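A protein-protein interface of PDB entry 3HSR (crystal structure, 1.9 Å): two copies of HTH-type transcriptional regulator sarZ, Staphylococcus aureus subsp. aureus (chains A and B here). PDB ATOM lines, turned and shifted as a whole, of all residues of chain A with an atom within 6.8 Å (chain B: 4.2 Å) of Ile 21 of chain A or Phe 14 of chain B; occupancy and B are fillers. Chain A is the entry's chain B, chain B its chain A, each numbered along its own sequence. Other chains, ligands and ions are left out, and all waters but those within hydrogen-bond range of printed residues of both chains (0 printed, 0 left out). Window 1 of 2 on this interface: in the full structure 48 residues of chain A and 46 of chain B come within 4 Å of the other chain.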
ATOM      1  N   LEU A  13       1.145 -22.636 -26.717  1.00  0.00           N
ATOM      2  CA  LEU A  13      -0.175 -22.876 -26.131  1.00  0.00           C
ATOM      3  C   LEU A  13      -0.131 -23.864 -24.957  1.00  0.00           C
ATOM      4  O   LEU A  13      -0.856 -23.678 -23.950  1.00  0.00           O
ATOM      5  CB  LEU A  13      -1.180 -23.330 -27.199  1.00  0.00           C
ATOM      6  CG  LEU A  13      -1.590 -22.233 -28.213  1.00  0.00           C
ATOM      7  CD1 LEU A  13      -2.364 -22.821 -29.418  1.00  0.00           C
ATOM      8  CD2 LEU A  13      -2.429 -21.119 -27.581  1.00  0.00           C
ATOM      9  N   PHE A  14       0.718 -24.891 -25.057  1.00  0.00           N
ATOM     10  CA  PHE A  14       0.947 -25.745 -23.878  1.00  0.00           C
ATOM     11  C   PHE A  14       1.645 -24.964 -22.765  1.00  0.00           C
ATOM     12  O   PHE A  14       1.394 -25.198 -21.601  1.00  0.00           O
ATOM     13  CB  PHE A  14       1.771 -26.977 -24.210  1.00  0.00           C
ATOM     14  CG  PHE A  14       0.946 -28.139 -24.648  1.00  0.00           C
ATOM     15  CD1 PHE A  14       0.107 -28.776 -23.756  1.00  0.00           C
ATOM     16  CD2 PHE A  14       1.031 -28.602 -25.960  1.00  0.00           C
ATOM     17  CE1 PHE A  14      -0.629 -29.868 -24.156  1.00  0.00           C
ATOM     18  CE2 PHE A  14       0.310 -29.688 -26.357  1.00  0.00           C
ATOM     19  CZ  PHE A  14      -0.528 -30.308 -25.480  1.00  0.00           C
ATOM     20  N   VAL A  16       1.346 -21.686 -21.974  1.00  0.00           N
ATOM     21  CA  VAL A  16       0.374 -20.811 -21.297  1.00  0.00           C
ATOM     22  C   VAL A  16      -0.638 -21.597 -20.499  1.00  0.00           C
ATOM     23  O   VAL A  16      -0.869 -21.292 -19.333  1.00  0.00           O
ATOM     24  CB  VAL A  16      -0.350 -19.874 -22.269  1.00  0.00           C
ATOM     25  CG1 VAL A  16      -1.372 -18.964 -21.467  1.00  0.00           C
ATOM     26  CG2 VAL A  16       0.657 -18.968 -22.923  1.00  0.00           C
ATOM     27  N   SER A  17      -1.243 -22.600 -21.138  1.00  0.00           N
ATOM     28  CA  SER A  17      -2.256 -23.425 -20.493  1.00  0.00           C
ATOM     29  C   SER A  17      -1.723 -24.164 -19.246  1.00  0.00           C
ATOM     30  O   SER A  17      -2.330 -24.098 -18.183  1.00  0.00           O
ATOM     31  CB  SER A  17      -2.907 -24.393 -21.506  1.00  0.00           C
ATOM     32  OG  SER A  17      -1.931 -25.056 -22.288  1.00  0.00           O
ATOM     33  N   SER A  18      -0.587 -24.868 -19.369  1.00  0.00           N
ATOM     34  CA  SER A  18       0.029 -25.580 -18.245  1.00  0.00           C
ATOM     35  C   SER A  18       0.347 -24.648 -17.074  1.00  0.00           C
ATOM     36  O   SER A  18      -0.025 -24.902 -15.922  1.00  0.00           O
ATOM     37  CB  SER A  18       1.326 -26.256 -18.707  1.00  0.00           C
ATOM     38  OG  SER A  18       2.042 -26.765 -17.594  1.00  0.00           O
ATOM     39  N   LYS A  19       1.048 -23.565 -17.388  1.00  0.00           N
ATOM     40  CA  LYS A  19       1.398 -22.515 -16.443  1.00  0.00           C
ATOM     41  C   LYS A  19       0.164 -22.134 -15.591  1.00  0.00           C
ATOM     42  O   LYS A  19       0.205 -22.024 -14.361  1.00  0.00           O
ATOM     43  CB  LYS A  19       1.815 -21.323 -17.307  1.00  0.00           C
ATOM     44  CG  LYS A  19       2.314 -20.116 -16.645  1.00  0.00           C
ATOM     45  CD  LYS A  19       3.113 -19.293 -17.668  1.00  0.00           C
ATOM     46  CE  LYS A  19       2.251 -18.193 -18.244  1.00  0.00           C
ATOM     47  NZ  LYS A  19       1.752 -17.337 -17.131  1.00  0.00           N
ATOM     48  N   GLU A  20      -0.937 -21.886 -16.290  1.00  0.00           N
ATOM     49  CA  GLU A  20      -2.122 -21.273 -15.687  1.00  0.00           C
ATOM     50  C   GLU A  20      -2.990 -22.296 -14.930  1.00  0.00           C
ATOM     51  O   GLU A  20      -3.518 -22.014 -13.862  1.00  0.00           O
ATOM     52  CB  GLU A  20      -2.922 -20.580 -16.787  1.00  0.00           C
ATOM     53  CG  GLU A  20      -2.178 -19.351 -17.367  1.00  0.00           C
ATOM     54  CD  GLU A  20      -2.046 -18.250 -16.324  1.00  0.00           C
ATOM     55  OE1 GLU A  20      -2.994 -18.100 -15.528  1.00  0.00           O
ATOM     56  OE2 GLU A  20      -0.997 -17.553 -16.276  1.00  0.00           O
ATOM     57  N   ILE A  21      -3.097 -23.495 -15.475  1.00  0.00           N
ATOM     58  CA  ILE A  21      -3.748 -24.578 -14.756  1.00  0.00           C
ATOM     59  C   ILE A  21      -3.017 -24.888 -13.445  1.00  0.00           C
ATOM     60  O   ILE A  21      -3.629 -24.898 -12.376  1.00  0.00           O
ATOM     61  CB  ILE A  21      -3.845 -25.806 -15.656  1.00  0.00           C
ATOM     62  CG1 ILE A  21      -4.820 -25.496 -16.807  1.00  0.00           C
ATOM     63  CG2 ILE A  21      -4.230 -27.046 -14.854  1.00  0.00           C
ATOM     64  CD1 ILE A  21      -4.764 -26.522 -17.923  1.00  0.00           C
ATOM     65  N   ILE A  22      -1.704 -25.077 -13.507  1.00  0.00           N
ATOM     66  CA  ILE A  22      -0.926 -25.336 -12.297  1.00  0.00           C
ATOM     67  C   ILE A  22      -1.110 -24.210 -11.252  1.00  0.00           C
ATOM     68  O   ILE A  22      -1.159 -24.463 -10.051  1.00  0.00           O
ATOM     69  CB  ILE A  22       0.564 -25.502 -12.632  1.00  0.00           C
ATOM     70  CG1 ILE A  22       0.802 -26.875 -13.275  1.00  0.00           C
ATOM     71  CG2 ILE A  22       1.439 -25.329 -11.389  1.00  0.00           C
ATOM     72  CD1 ILE A  22       2.125 -26.953 -14.053  1.00  0.00           C
ATOM     73  N   LYS A  23      -1.188 -22.969 -11.720  1.00  0.00           N
ATOM     74  CA  LYS A  23      -1.372 -21.835 -10.821  1.00  0.00           C
ATOM     75  C   LYS A  23      -2.650 -22.026  -9.990  1.00  0.00           C
ATOM     76  O   LYS A  23      -2.653 -21.830  -8.761  1.00  0.00           O
ATOM     77  CB  LYS A  23      -1.396 -20.517 -11.628  1.00  0.00           C
ATOM     78  CG  LYS A  23      -1.026 -19.274 -10.824  1.00  0.00           C
ATOM     79  CD  LYS A  23      -1.237 -17.975 -11.638  1.00  0.00           C
ATOM     80  CE  LYS A  23      -0.385 -17.963 -12.904  1.00  0.00           C
ATOM     81  NZ  LYS A  23      -0.646 -16.760 -13.767  1.00  0.00           N
ATOM     82  N   LYS A  24      -3.737 -22.431 -10.636  1.00  0.00           N
ATOM     83  CA  LYS A  24      -4.992 -22.601  -9.922  1.00  0.00           C
ATOM     84  C   LYS A  24      -4.930 -23.748  -8.913  1.00  0.00           C
ATOM     85  O   LYS A  24      -5.528 -23.677  -7.846  1.00  0.00           O
ATOM     86  CB  LYS A  24      -6.168 -22.778 -10.883  1.00  0.00           C
ATOM     87  CG  LYS A  24      -6.533 -21.474 -11.582  1.00  0.00           C
ATOM     88  CD  LYS A  24      -7.977 -21.416 -11.991  1.00  0.00           C
ATOM     89  CE  LYS A  24      -8.243 -20.094 -12.680  1.00  0.00           C
ATOM     90  NZ  LYS A  24      -8.449 -19.037 -11.666  1.00  0.00           N
ATOM     91  N   TYR A  25      -4.197 -24.809  -9.234  1.00  0.00           N
ATOM     92  CA  TYR A  25      -4.076 -25.905  -8.268  1.00  0.00           C
ATOM     93  C   TYR A  25      -3.291 -25.423  -7.077  1.00  0.00           C
ATOM     94  O   TYR A  25      -3.670 -25.644  -5.926  1.00  0.00           O
ATOM     95  CB  TYR A  25      -3.342 -27.079  -8.889  1.00  0.00           C
ATOM     96  CG  TYR A  25      -4.232 -28.014  -9.626  1.00  0.00           C
ATOM     97  CD1 TYR A  25      -4.472 -27.853 -10.990  1.00  0.00           C
ATOM     98  CD2 TYR A  25      -4.849 -29.054  -8.962  1.00  0.00           C
ATOM     99  CE1 TYR A  25      -5.298 -28.722 -11.672  1.00  0.00           C
ATOM    100  CE2 TYR A  25      -5.667 -29.922  -9.627  1.00  0.00           C
ATOM    101  CZ  TYR A  25      -5.875 -29.766 -10.984  1.00  0.00           C
ATOM    102  OH  TYR A  25      -6.715 -30.645 -11.615  1.00  0.00           O
ATOM    103  N   THR A  26      -2.177 -24.766  -7.377  1.00  0.00           N
ATOM    104  CA  THR A  26      -1.247 -24.341  -6.366  1.00  0.00           C
ATOM    105  C   THR A  26      -1.961 -23.447  -5.383  1.00  0.00           C
ATOM    106  O   THR A  26      -1.696 -23.507  -4.198  1.00  0.00           O
ATOM    107  CB  THR A  26      -0.045 -23.632  -6.983  1.00  0.00           C
ATOM    108  OG1 THR A  26       0.692 -24.581  -7.757  1.00  0.00           O
ATOM    109  CG2 THR A  26       0.865 -23.090  -5.898  1.00  0.00           C
ATOM    110  N   TYR A  36       2.088 -28.999  -6.275  1.00  0.00           N
ATOM    111  CA  TYR A  36       1.298 -29.630  -7.324  1.00  0.00           C
ATOM    112  C   TYR A  36       1.771 -31.078  -7.634  1.00  0.00           C
ATOM    113  O   TYR A  36       0.975 -32.022  -7.733  1.00  0.00           O
ATOM    114  CB  TYR A  36       1.382 -28.749  -8.576  1.00  0.00           C
ATOM    115  CG  TYR A  36       0.707 -29.335  -9.773  1.00  0.00           C
ATOM    116  CD1 TYR A  36      -0.684 -29.460  -9.819  1.00  0.00           C
ATOM    117  CD2 TYR A  36       1.451 -29.769 -10.859  1.00  0.00           C
ATOM    118  CE1 TYR A  36      -1.305 -29.997 -10.935  1.00  0.00           C
ATOM    119  CE2 TYR A  36       0.847 -30.310 -11.972  1.00  0.00           C
ATOM    120  CZ  TYR A  36      -0.533 -30.417 -12.001  1.00  0.00           C
ATOM    121  OH  TYR A  36      -1.142 -30.957 -13.111  1.00  0.00           O
ATOM    122  N   VAL A 114     -11.128 -26.633  -9.883  1.00  0.00           N
ATOM    123  CA  VAL A 114     -10.386 -25.968 -10.923  1.00  0.00           C
ATOM    124  C   VAL A 114     -11.170 -25.964 -12.239  1.00  0.00           C
ATOM    125  O   VAL A 114     -11.243 -24.949 -12.936  1.00  0.00           O
ATOM    126  CB  VAL A 114      -8.981 -26.578 -11.103  1.00  0.00           C
ATOM    127  CG1 VAL A 114      -8.271 -25.993 -12.317  1.00  0.00           C
ATOM    128  CG2 VAL A 114      -8.157 -26.348  -9.837  1.00  0.00           C
ATOM    129  N   PHE A 118     -12.715 -22.618 -14.545  1.00  0.00           N
ATOM    130  CA  PHE A 118     -12.388 -22.250 -15.904  1.00  0.00           C
ATOM    131  C   PHE A 118     -13.620 -22.181 -16.800  1.00  0.00           C
ATOM    132  O   PHE A 118     -14.592 -22.927 -16.638  1.00  0.00           O
ATOM    133  CB  PHE A 118     -11.372 -23.234 -16.520  1.00  0.00           C
ATOM    134  CG  PHE A 118      -9.961 -22.983 -16.083  1.00  0.00           C
ATOM    135  CD1 PHE A 118      -9.226 -23.971 -15.461  1.00  0.00           C
ATOM    136  CD2 PHE A 118      -9.368 -21.753 -16.302  1.00  0.00           C
ATOM    137  CE1 PHE A 118      -7.918 -23.735 -15.078  1.00  0.00           C
ATOM    138  CE2 PHE A 118      -8.058 -21.507 -15.903  1.00  0.00           C
ATOM    139  CZ  PHE A 118      -7.333 -22.500 -15.296  1.00  0.00           C
ATOM    140  N   ILE A 120     -14.836 -23.406 -19.716  1.00  0.00           N
ATOM    141  CA  ILE A 120     -14.567 -24.503 -20.612  1.00  0.00           C
ATOM    142  C   ILE A 120     -15.773 -25.343 -20.428  1.00  0.00           C
ATOM    143  O   ILE A 120     -16.186 -25.588 -19.282  1.00  0.00           O
ATOM    144  CB  ILE A 120     -13.278 -25.277 -20.211  1.00  0.00           C
ATOM    145  CG1 ILE A 120     -12.979 -26.361 -21.257  1.00  0.00           C
ATOM    146  CG2 ILE A 120     -13.411 -25.883 -18.767  1.00  0.00           C
ATOM    147  CD1 ILE A 120     -11.955 -27.388 -20.800  1.00  0.00           C
ATOM    148  N   ILE A 128     -10.704 -32.116 -25.669  1.00  0.00           N
ATOM    149  CA  ILE A 128      -9.345 -32.033 -25.151  1.00  0.00           C
ATOM    150  C   ILE A 128      -8.927 -33.402 -24.620  1.00  0.00           C
ATOM    151  O   ILE A 128      -7.834 -33.883 -24.941  1.00  0.00           O
ATOM    152  CB  ILE A 128      -9.185 -30.951 -24.066  1.00  0.00           C
ATOM    153  CG1 ILE A 128      -9.257 -29.544 -24.716  1.00  0.00           C
ATOM    154  CG2 ILE A 128      -7.838 -31.119 -23.361  1.00  0.00           C
ATOM    155  CD1 ILE A 128      -9.461 -28.375 -23.722  1.00  0.00           C
ATOM    156  N   LEU A 132      -5.737 -35.384 -26.158  1.00  0.00           N
ATOM    157  CA  LEU A 132      -4.524 -35.579 -25.364  1.00  0.00           C
ATOM    158  C   LEU A 132      -4.274 -37.077 -25.119  1.00  0.00           C
ATOM    159  O   LEU A 132      -3.131 -37.508 -25.026  1.00  0.00           O
ATOM    160  CB  LEU A 132      -4.518 -34.778 -24.058  1.00  0.00           C
ATOM    161  CG  LEU A 132      -4.557 -33.259 -24.252  1.00  0.00           C
ATOM    162  CD1 LEU A 132      -4.525 -32.502 -22.952  1.00  0.00           C
ATOM    163  CD2 LEU A 132      -3.415 -32.796 -25.182  1.00  0.00           C
ATOM    164  N   LEU B  10      -8.993 -34.736 -17.471  1.00  0.00           N
ATOM    165  CA  LEU B  10      -8.436 -33.502 -17.965  1.00  0.00           C
ATOM    166  C   LEU B  10      -7.284 -33.018 -17.080  1.00  0.00           C
ATOM    167  O   LEU B  10      -6.279 -32.515 -17.576  1.00  0.00           O
ATOM    168  CB  LEU B  10      -9.574 -32.451 -18.085  1.00  0.00           C
ATOM    169  CG  LEU B  10      -9.444 -31.158 -18.872  1.00  0.00           C
ATOM    170  CD1 LEU B  10      -9.395 -31.421 -20.333  1.00  0.00           C
ATOM    171  CD2 LEU B  10     -10.674 -30.248 -18.533  1.00  0.00           C
ATOM    172  N   CYS B  11      -7.421 -33.150 -15.768  1.00  0.00           N
ATOM    173  CA  CYS B  11      -6.317 -32.831 -14.861  1.00  0.00           C
ATOM    174  C   CYS B  11      -5.082 -33.651 -15.291  1.00  0.00           C
ATOM    175  O   CYS B  11      -4.021 -33.105 -15.629  1.00  0.00           O
ATOM    176  CB  CYS B  11      -6.744 -33.164 -13.419  1.00  0.00           C
ATOM    177  SG  CYS B  11      -5.617 -32.818 -11.969  1.00  0.00           S
ATOM    178  N   PHE B  12      -5.249 -34.970 -15.316  1.00  0.00           N
ATOM    179  CA  PHE B  12      -4.113 -35.859 -15.511  1.00  0.00           C
ATOM    180  C   PHE B  12      -3.511 -35.806 -16.931  1.00  0.00           C
ATOM    181  O   PHE B  12      -2.288 -35.683 -17.098  1.00  0.00           O
ATOM    182  CB  PHE B  12      -4.474 -37.279 -15.119  1.00  0.00           C
ATOM    183  CG  PHE B  12      -3.279 -38.155 -14.988  1.00  0.00           C
ATOM    184  CD1 PHE B  12      -2.408 -37.997 -13.916  1.00  0.00           C
ATOM    185  CD2 PHE B  12      -2.997 -39.105 -15.947  1.00  0.00           C
ATOM    186  CE1 PHE B  12      -1.285 -38.787 -13.795  1.00  0.00           C
ATOM    187  CE2 PHE B  12      -1.873 -39.892 -15.840  1.00  0.00           C
ATOM    188  CZ  PHE B  12      -1.012 -39.736 -14.766  1.00  0.00           C
ATOM    189  N   LEU B  13      -4.363 -35.888 -17.949  1.00  0.00           N
ATOM    190  CA  LEU B  13      -3.865 -35.845 -19.313  1.00  0.00           C
ATOM    191  C   LEU B  13      -3.069 -34.576 -19.615  1.00  0.00           C
ATOM    192  O   LEU B  13      -2.178 -34.604 -20.461  1.00  0.00           O
ATOM    193  CB  LEU B  13      -4.987 -36.036 -20.339  1.00  0.00           C
ATOM    194  CG  LEU B  13      -5.539 -37.451 -20.360  1.00  0.00           C
ATOM    195  CD1 LEU B  13      -6.657 -37.537 -21.386  1.00  0.00           C
ATOM    196  CD2 LEU B  13      -4.436 -38.456 -20.683  1.00  0.00           C
ATOM    197  N   PHE B  14      -3.390 -33.471 -18.938  1.00  0.00           N
ATOM    198  CA  PHE B  14      -2.666 -32.233 -19.122  1.00  0.00           C
ATOM    199  C   PHE B  14      -1.356 -32.246 -18.398  1.00  0.00           C
ATOM    200  O   PHE B  14      -0.358 -31.678 -18.875  1.00  0.00           O
ATOM    201  CB  PHE B  14      -3.469 -31.062 -18.554  1.00  0.00           C
ATOM    202  CG  PHE B  14      -3.870 -30.073 -19.570  1.00  0.00           C
ATOM    203  CD1 PHE B  14      -2.915 -29.304 -20.187  1.00  0.00           C
ATOM    204  CD2 PHE B  14      -5.198 -29.897 -19.904  1.00  0.00           C
ATOM    205  CE1 PHE B  14      -3.247 -28.381 -21.132  1.00  0.00           C
ATOM    206  CE2 PHE B  14      -5.555 -28.965 -20.865  1.00  0.00           C
ATOM    207  CZ  PHE B  14      -4.567 -28.202 -21.478  1.00  0.00           C
ATOM    208  N   TYR B  15      -1.390 -32.817 -17.200  1.00  0.00           N
ATOM    209  CA  TYR B  15      -0.205 -32.985 -16.411  1.00  0.00           C
ATOM    210  C   TYR B  15       0.813 -33.771 -17.235  1.00  0.00           C
ATOM    211  O   TYR B  15       1.990 -33.401 -17.279  1.00  0.00           O
ATOM    212  CB  TYR B  15      -0.520 -33.729 -15.118  1.00  0.00           C
ATOM    213  CG  TYR B  15       0.685 -34.315 -14.457  1.00  0.00           C
ATOM    214  CD1 TYR B  15       1.538 -33.511 -13.725  1.00  0.00           C
ATOM    215  CD2 TYR B  15       0.998 -35.682 -14.576  1.00  0.00           C
ATOM    216  CE1 TYR B  15       2.641 -34.017 -13.126  1.00  0.00           C
ATOM    217  CE2 TYR B  15       2.125 -36.209 -13.971  1.00  0.00           C
ATOM    218  CZ  TYR B  15       2.941 -35.370 -13.251  1.00  0.00           C
ATOM    219  OH  TYR B  15       4.050 -35.844 -12.617  1.00  0.00           O
ATOM    220  N   VAL B  16       0.351 -34.851 -17.868  1.00  0.00           N
ATOM    221  CA  VAL B  16       1.261 -35.774 -18.549  1.00  0.00           C
ATOM    222  C   VAL B  16       1.844 -35.132 -19.798  1.00  0.00           C
ATOM    223  O   VAL B  16       3.032 -35.228 -20.032  1.00  0.00           O
ATOM    224  CB  VAL B  16       0.576 -37.069 -18.939  1.00  0.00           C
ATOM    225  CG1 VAL B  16       1.455 -37.839 -19.956  1.00  0.00           C
ATOM    226  CG2 VAL B  16       0.286 -37.897 -17.689  1.00  0.00           C
ATOM    227  N   SER B  17       0.995 -34.467 -20.582  1.00  0.00           N
ATOM    228  CA  SER B  17       1.434 -33.721 -21.775  1.00  0.00           C
ATOM    229  C   SER B  17       2.574 -32.708 -21.476  1.00  0.00           C
ATOM    230  O   SER B  17       3.615 -32.709 -22.157  1.00  0.00           O
ATOM    231  CB  SER B  17       0.239 -33.011 -22.412  1.00  0.00           C
ATOM    232  OG  SER B  17      -0.726 -33.960 -22.872  1.00  0.00           O
ATOM    233  N   SER B  18       2.385 -31.890 -20.435  1.00  0.00           N
ATOM    234  CA  SER B  18       3.318 -30.833 -20.082  1.00  0.00           C
ATOM    235  C   SER B  18       4.576 -31.432 -19.488  1.00  0.00           C
ATOM    236  O   SER B  18       5.689 -30.915 -19.666  1.00  0.00           O
ATOM    237  CB  SER B  18       2.666 -29.885 -19.069  1.00  0.00           C
ATOM    238  OG  SER B  18       3.632 -29.054 -18.449  1.00  0.00           O
ATOM    239  N   LEU B 132      -6.716 -25.743 -27.586  1.00  0.00           N
ATOM    240  CA  LEU B 132      -5.964 -24.984 -26.612  1.00  0.00           C
ATOM    241  C   LEU B 132      -6.041 -23.506 -26.874  1.00  0.00           C
ATOM    242  O   LEU B 132      -6.018 -22.721 -25.947  1.00  0.00           O
ATOM    243  CB  LEU B 132      -4.474 -25.366 -26.598  1.00  0.00           C
ATOM    244  CG  LEU B 132      -4.164 -26.821 -26.211  1.00  0.00           C
ATOM    245  CD1 LEU B 132      -2.672 -27.031 -26.245  1.00  0.00           C
ATOM    246  CD2 LEU B 132      -4.736 -27.059 -24.823  1.00  0.00           C
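Leu 13 of chain A touches Leu 132 of chain B, and with the chains exchanged Leu 132 of chain A touches Leu 13 of chain B.
Phe 14 of chain A touches Leu 132 of chain B, but with the chains exchanged Leu 132 of chain A does not touch Phe 14 of chain B (4.1 Å).
Ser 18 of chain B touches its own counterpart, Ser 18 of chain A.
Leu 132 of chain A touches Ser 17 of chain B, but with the chains exchanged Ser 17 of chain A does not touch Leu 132 of chain B (4.3 Å).
Positions printed for both chains: 13, 14, 16, 17, 18 and 132.
Of the 12 pairs that touch across the chains among the printed residues, 5 have their exchanged pair printed and touching as well.
The side-chain hydroxyl of Ser 17 of chain B is in hydrogen-bond range of the backbone carbonyl oxygen of Leu 13 of chain B, at 2.9 Å.
The backbone carbonyl oxygen (O) of Leu 13 of chain A sits at hydrogen-bond distance from the side-chain hydroxyl (OG) of Ser 17 of chain A (2.4 Å).
The backbone carbonyl oxygen (O) of Phe 14 of chain A sits close to the side-chain hydroxyl (OG) of Ser 17 of chain A (3.4 Å).
Printed residues of chain B within 4 Å of Ile 128 of chain A: Leu 10 (3.4 Å).
Of the printed residues of chain B, Phe 14 of chain A touches Ser 17 and Leu 132.
Of the printed residues of chain B, Ser 18 of chain A touches Ser 18.
Printed residues of chain B within 4 Å of Leu 13 of chain A: Leu 132.
Printed residues of chain A within 4 Å of Tyr 15 of chain B: Tyr 36.
Ile 22 of chain A touches none of the printed residues of chain B.
Val 16 of chain B touches none of the printed residues of chain A.
Among the printed residues, merely in contact across the chains: Leu 13 of chain A with Leu 132 of chain B, Phe 14 of chain A with Ser 17 of chain B, Phe 14 of chain A with Leu 132 of chain B, Ser 17 of chain A with Phe 14 of chain B, Ile 21 of chain A with Phe 14 of chain B, Tyr 36 of chain A with Tyr 15 of chain B, Ile 120 of chain A with Leu 10 of chain B, Ile 128 of chain A with Leu 10 of chain B, Leu 132 of chain A with Leu 13 of chain B and Leu 132 of chain A with Ser 17 of chain B.
Printed residues of chain B that touch a printed residue of chain A: Leu 10, Cys 11, Leu 13, Phe 14, Tyr 15, Ser 17, Ser 18 and Leu 132.
Among the printed residues, 12 pairs touch across the chains.
Among the printed residues, no Asp or Glu carboxylate lies within 4 Å of a Lys or Arg side-chain nitrogen of the other chain.
SG of Cys 11 of chain B is in hydrogen-bond range of OH of Tyr 25 of chain A, at 2.5 Å.
OG of Ser 18 of chain A sits at hydrogen-bond distance from OG of Ser 18 of chain B (2.9 Å).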
